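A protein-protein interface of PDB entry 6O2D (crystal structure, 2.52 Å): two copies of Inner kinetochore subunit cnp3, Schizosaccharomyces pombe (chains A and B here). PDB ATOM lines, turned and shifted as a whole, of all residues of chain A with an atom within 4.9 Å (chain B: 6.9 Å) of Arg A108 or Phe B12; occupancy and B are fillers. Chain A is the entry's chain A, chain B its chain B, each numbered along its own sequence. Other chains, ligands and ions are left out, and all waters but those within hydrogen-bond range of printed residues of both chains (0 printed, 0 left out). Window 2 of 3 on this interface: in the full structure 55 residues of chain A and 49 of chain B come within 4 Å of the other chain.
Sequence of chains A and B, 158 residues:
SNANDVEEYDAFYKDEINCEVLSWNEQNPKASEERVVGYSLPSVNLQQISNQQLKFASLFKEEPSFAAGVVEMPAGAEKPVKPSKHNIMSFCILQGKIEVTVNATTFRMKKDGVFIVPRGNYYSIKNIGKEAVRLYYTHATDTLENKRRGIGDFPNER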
ATOM      1  N   ILE A  98      -3.381  29.391 -12.096  1.00  0.00           N
ATOM      2  CA  ILE A  98      -3.763  28.518 -13.195  1.00  0.00           C
ATOM      3  C   ILE A  98      -4.952  27.654 -12.803  1.00  0.00           C
ATOM      4  O   ILE A  98      -5.237  27.426 -11.624  1.00  0.00           O
ATOM      5  CB  ILE A  98      -2.602  27.607 -13.663  1.00  0.00           C
ATOM      6  CG1 ILE A  98      -2.190  26.635 -12.552  1.00  0.00           C
ATOM      7  CG2 ILE A  98      -1.423  28.432 -14.117  1.00  0.00           C
ATOM      8  CD1 ILE A  98      -1.008  25.750 -12.916  1.00  0.00           C
ATOM      9  N   GLU A  99      -5.664  27.205 -13.829  1.00  0.00           N
ATOM     10  CA  GLU A  99      -6.661  26.152 -13.729  1.00  0.00           C
ATOM     11  C   GLU A  99      -6.160  24.970 -14.544  1.00  0.00           C
ATOM     12  O   GLU A  99      -5.779  25.134 -15.710  1.00  0.00           O
ATOM     13  CB  GLU A  99      -8.021  26.647 -14.234  1.00  0.00           C
ATOM     14  CG  GLU A  99      -9.062  25.569 -14.476  1.00  0.00           C
ATOM     15  CD  GLU A  99     -10.280  26.105 -15.207  1.00  0.00           C
ATOM     16  OE1 GLU A  99     -10.927  27.046 -14.688  1.00  0.00           O
ATOM     17  OE2 GLU A  99     -10.583  25.590 -16.305  1.00  0.00           O
ATOM     18  N   THR A 106     -11.008  19.447 -13.103  1.00  0.00           N
ATOM     19  CA  THR A 106     -10.308  20.726 -13.093  1.00  0.00           C
ATOM     20  C   THR A 106     -10.090  21.201 -11.661  1.00  0.00           C
ATOM     21  O   THR A 106     -10.946  21.018 -10.792  1.00  0.00           O
ATOM     22  CB  THR A 106     -11.064  21.799 -13.886  1.00  0.00           C
ATOM     23  OG1 THR A 106     -12.189  22.246 -13.127  1.00  0.00           O
ATOM     24  CG2 THR A 106     -11.542  21.246 -15.232  1.00  0.00           C
ATOM     25  N   PHE A 107      -8.922  21.794 -11.422  1.00  0.00           N
ATOM     26  CA  PHE A 107      -8.538  22.297 -10.113  1.00  0.00           C
ATOM     27  C   PHE A 107      -7.702  23.551 -10.320  1.00  0.00           C
ATOM     28  O   PHE A 107      -7.025  23.712 -11.342  1.00  0.00           O
ATOM     29  CB  PHE A 107      -7.776  21.258  -9.270  1.00  0.00           C
ATOM     30  CG  PHE A 107      -6.610  20.601  -9.975  1.00  0.00           C
ATOM     31  CD1 PHE A 107      -5.316  21.077  -9.801  1.00  0.00           C
ATOM     32  CD2 PHE A 107      -6.801  19.482 -10.771  1.00  0.00           C
ATOM     33  CE1 PHE A 107      -4.247  20.467 -10.419  1.00  0.00           C
ATOM     34  CE2 PHE A 107      -5.727  18.866 -11.393  1.00  0.00           C
ATOM     35  CZ  PHE A 107      -4.455  19.358 -11.215  1.00  0.00           C
ATOM     36  N   ARG A 108      -7.732  24.426  -9.323  1.00  0.00           N
ATOM     37  CA  ARG A 108      -7.046  25.708  -9.379  1.00  0.00           C
ATOM     38  C   ARG A 108      -5.829  25.706  -8.477  1.00  0.00           C
ATOM     39  O   ARG A 108      -5.880  25.201  -7.350  1.00  0.00           O
ATOM     40  CB  ARG A 108      -7.971  26.845  -8.944  1.00  0.00           C
ATOM     41  CG  ARG A 108      -8.960  27.300  -9.988  1.00  0.00           C
ATOM     42  CD  ARG A 108      -9.874  28.365  -9.406  1.00  0.00           C
ATOM     43  NE  ARG A 108     -10.481  27.900  -8.163  1.00  0.00           N
ATOM     44  CZ  ARG A 108     -11.728  27.453  -8.065  1.00  0.00           C
ATOM     45  NH1 ARG A 108     -12.192  27.040  -6.893  1.00  0.00           N
ATOM     46  NH2 ARG A 108     -12.507  27.420  -9.136  1.00  0.00           N
ATOM     47  N   MET A 109      -4.754  26.313  -8.964  1.00  0.00           N
ATOM     48  CA  MET A 109      -3.519  26.383  -8.209  1.00  0.00           C
ATOM     49  C   MET A 109      -2.805  27.680  -8.480  1.00  0.00           C
ATOM     50  O   MET A 109      -3.101  28.361  -9.468  1.00  0.00           O
ATOM     51  CB  MET A 109      -2.632  25.191  -8.541  1.00  0.00           C
ATOM     52  CG  MET A 109      -3.018  23.983  -7.741  1.00  0.00           C
ATOM     53  SD  MET A 109      -1.789  22.564  -8.124  1.00  0.00           S
ATOM     54  CE  MET A 109      -1.438  22.070  -6.294  1.00  0.00           C
ATOM     55  N   LYS A 110      -1.867  28.025  -7.606  1.00  0.00           N
ATOM     56  CA  LYS A 110      -1.212  29.326  -7.674  1.00  0.00           C
ATOM     57  C   LYS A 110       0.244  29.159  -7.261  1.00  0.00           C
ATOM     58  O   LYS A 110       0.779  28.044  -7.211  1.00  0.00           O
ATOM     59  CB  LYS A 110      -1.955  30.338  -6.786  1.00  0.00           C
ATOM     60  CG  LYS A 110      -2.085  29.907  -5.326  1.00  0.00           C
ATOM     61  CD  LYS A 110      -2.637  31.037  -4.447  1.00  0.00           C
ATOM     62  CE  LYS A 110      -3.108  30.507  -3.092  1.00  0.00           C
ATOM     63  NZ  LYS A 110      -2.080  29.629  -2.441  1.00  0.00           N
ATOM     64  N   ILE A 128      -5.625  31.771 -15.398  1.00  0.00           N
ATOM     65  CA  ILE A 128      -6.859  32.395 -14.923  1.00  0.00           C
ATOM     66  C   ILE A 128      -6.588  33.706 -14.197  1.00  0.00           C
ATOM     67  O   ILE A 128      -7.485  34.235 -13.533  1.00  0.00           O
ATOM     68  CB  ILE A 128      -7.654  31.446 -14.010  1.00  0.00           C
ATOM     69  CG1 ILE A 128      -6.801  31.045 -12.809  1.00  0.00           C
ATOM     70  CG2 ILE A 128      -8.146  30.230 -14.771  1.00  0.00           C
ATOM     71  CD1 ILE A 128      -7.479  30.087 -11.873  1.00  0.00           C
ATOM     72  N   TYR B   9      -8.939  34.898  -4.237  1.00  0.00           N
ATOM     73  CA  TYR B   9      -9.439  34.527  -2.917  1.00  0.00           C
ATOM     74  C   TYR B   9      -8.772  33.239  -2.445  1.00  0.00           C
ATOM     75  O   TYR B   9      -8.875  32.205  -3.107  1.00  0.00           O
ATOM     76  CB  TYR B   9     -10.961  34.370  -2.945  1.00  0.00           C
ATOM     77  CG  TYR B   9     -11.717  35.631  -2.592  1.00  0.00           C
ATOM     78  CD1 TYR B   9     -13.089  35.714  -2.773  1.00  0.00           C
ATOM     79  CD2 TYR B   9     -11.058  36.735  -2.065  1.00  0.00           C
ATOM     80  CE1 TYR B   9     -13.785  36.865  -2.453  1.00  0.00           C
ATOM     81  CE2 TYR B   9     -11.747  37.891  -1.737  1.00  0.00           C
ATOM     82  CZ  TYR B   9     -13.109  37.951  -1.932  1.00  0.00           C
ATOM     83  OH  TYR B   9     -13.796  39.100  -1.608  1.00  0.00           O
ATOM     84  N   ASP B  10      -8.085  33.306  -1.298  1.00  0.00           N
ATOM     85  CA  ASP B  10      -7.273  32.179  -0.842  1.00  0.00           C
ATOM     86  C   ASP B  10      -8.098  30.924  -0.587  1.00  0.00           C
ATOM     87  O   ASP B  10      -7.548  29.816  -0.625  1.00  0.00           O
ATOM     88  CB  ASP B  10      -6.506  32.560   0.428  1.00  0.00           C
ATOM     89  CG  ASP B  10      -5.122  31.924   0.490  1.00  0.00           C
ATOM     90  OD1 ASP B  10      -4.331  32.114  -0.460  1.00  0.00           O
ATOM     91  OD2 ASP B  10      -4.819  31.241   1.495  1.00  0.00           O
ATOM     92  N   ALA B  11      -9.403  31.066  -0.339  1.00  0.00           N
ATOM     93  CA  ALA B  11     -10.247  29.926  -0.001  1.00  0.00           C
ATOM     94  C   ALA B  11     -10.542  29.023  -1.193  1.00  0.00           C
ATOM     95  O   ALA B  11     -10.955  27.877  -0.990  1.00  0.00           O
ATOM     96  CB  ALA B  11     -11.560  30.412   0.621  1.00  0.00           C
ATOM     97  N   PHE B  12     -10.326  29.495  -2.420  1.00  0.00           N
ATOM     98  CA  PHE B  12     -10.658  28.738  -3.619  1.00  0.00           C
ATOM     99  C   PHE B  12      -9.482  27.939  -4.169  1.00  0.00           C
ATOM    100  O   PHE B  12      -9.593  27.383  -5.266  1.00  0.00           O
ATOM    101  CB  PHE B  12     -11.201  29.681  -4.693  1.00  0.00           C
ATOM    102  CG  PHE B  12     -12.594  30.172  -4.417  1.00  0.00           C
ATOM    103  CD1 PHE B  12     -13.696  29.381  -4.697  1.00  0.00           C
ATOM    104  CD2 PHE B  12     -12.801  31.421  -3.850  1.00  0.00           C
ATOM    105  CE1 PHE B  12     -14.983  29.847  -4.442  1.00  0.00           C
ATOM    106  CE2 PHE B  12     -14.083  31.883  -3.586  1.00  0.00           C
ATOM    107  CZ  PHE B  12     -15.174  31.095  -3.876  1.00  0.00           C
ATOM    108  N   TYR B  13      -8.372  27.857  -3.428  1.00  0.00           N
ATOM    109  CA  TYR B  13      -7.146  27.178  -3.856  1.00  0.00           C
ATOM    110  C   TYR B  13      -6.839  26.077  -2.848  1.00  0.00           C
ATOM    111  O   TYR B  13      -6.306  26.346  -1.769  1.00  0.00           O
ATOM    112  CB  TYR B  13      -5.998  28.168  -3.967  1.00  0.00           C
ATOM    113  CG  TYR B  13      -6.119  29.052  -5.173  1.00  0.00           C
ATOM    114  CD1 TYR B  13      -5.448  28.739  -6.348  1.00  0.00           C
ATOM    115  CD2 TYR B  13      -6.938  30.188  -5.153  1.00  0.00           C
ATOM    116  CE1 TYR B  13      -5.562  29.536  -7.465  1.00  0.00           C
ATOM    117  CE2 TYR B  13      -7.062  30.994  -6.272  1.00  0.00           C
ATOM    118  CZ  TYR B  13      -6.362  30.658  -7.425  1.00  0.00           C
ATOM    119  OH  TYR B  13      -6.455  31.435  -8.551  1.00  0.00           O
ATOM    120  N   LYS B  14      -7.167  24.840  -3.205  1.00  0.00           N
ATOM    121  CA  LYS B  14      -7.028  23.727  -2.280  1.00  0.00           C
ATOM    122  C   LYS B  14      -5.560  23.437  -1.957  1.00  0.00           C
ATOM    123  O   LYS B  14      -4.654  23.653  -2.774  1.00  0.00           O
ATOM    124  CB  LYS B  14      -7.705  22.483  -2.852  1.00  0.00           C
ATOM    125  CG  LYS B  14      -9.231  22.502  -2.792  1.00  0.00           C
ATOM    126  CD  LYS B  14      -9.825  21.260  -3.456  1.00  0.00           C
ATOM    127  CE  LYS B  14     -11.167  21.555  -4.111  1.00  0.00           C
ATOM    128  NZ  LYS B  14     -12.239  20.685  -3.552  1.00  0.00           N
ATOM    129  N   ILE B  17      -4.842  18.199  -3.681  1.00  0.00           N
ATOM    130  CA  ILE B  17      -5.771  17.925  -4.772  1.00  0.00           C
ATOM    131  C   ILE B  17      -5.830  16.422  -4.987  1.00  0.00           C
ATOM    132  O   ILE B  17      -4.850  15.812  -5.430  1.00  0.00           O
ATOM    133  CB  ILE B  17      -5.363  18.617  -6.078  1.00  0.00           C
ATOM    134  CG1 ILE B  17      -4.867  20.034  -5.808  1.00  0.00           C
ATOM    135  CG2 ILE B  17      -6.526  18.579  -7.070  1.00  0.00           C
ATOM    136  CD1 ILE B  17      -5.924  20.938  -5.299  1.00  0.00           C
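The backbone carbonyl oxygen (O) of Phe B12 is in hydrogen-bond range of the guanidinium group (NE) of Arg A108, 3.1 Å away. OD1 of Asp B10 is in salt-bridge range of NZ of Lys A110 (3.9 Å).
Of chain B, only Phe B12 (3.1 Å) and Tyr B13 (3.7 Å) come within 4 Å of Arg A108. Printed residues of chain B within 4 Å of Met A109: Tyr B13 (3.4 Å). Printed residues of chain B within 4 Å of Lys A110: Asp B10 and Tyr B13. Printed residues of chain B within 4 Å of Ile A128: Tyr B13 (3.7 Å). Of the printed residues of chain A, Asp B10 touches Lys A110 (3.3 Å). Phe B12 touches one residue of chain A. Printed residues of chain A within 4 Å of Tyr B13: Arg A108, Met A109, Lys A110 and Ile A128. Lys B14 touches none of the printed residues of chain A. The nearest residue of chain B that does not touch Arg A108 is Lys B14 (4.4 Å). The nearest printed residue of chain A that does not touch Phe B12 is Met A109 (6.2 Å). The nearest printed residue of chain B that does not touch Ile A128 is Phe B12 (7.4 Å).
Of the 8 printed residues of chain A, 5 touch a printed residue of chain B. Along chain A the printed residues that touch a printed residue of chain B span positions 107 to 128. Among the printed residues, 7 pairs touch across the chains. Among the printed residues, Asp or Glu carboxylates within 4 Å of a Lys or Arg side-chain nitrogen of the other chain: Lys A110 with Asp B10 (3.9 Å).
The backbone carbonyl oxygen (O) of Met A109 sits at hydrogen-bond distance from the backbone NH (N) of Ile A98.
CG2 of Ile B17 touches CG of Phe A107, at 3.5 Å. Arg A108 touches Tyr B13 (O to CD1, 3.7 Å). Met A109 touches Tyr B13 (O to CE1, 3.4 Å). Tyr B13 touches Lys A110. Tyr B13 touches Ile A128.
No position is printed for both chains. Of the 7 pairs that touch across the chains among the printed residues, none has its exchanged pair printed and touching as well.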
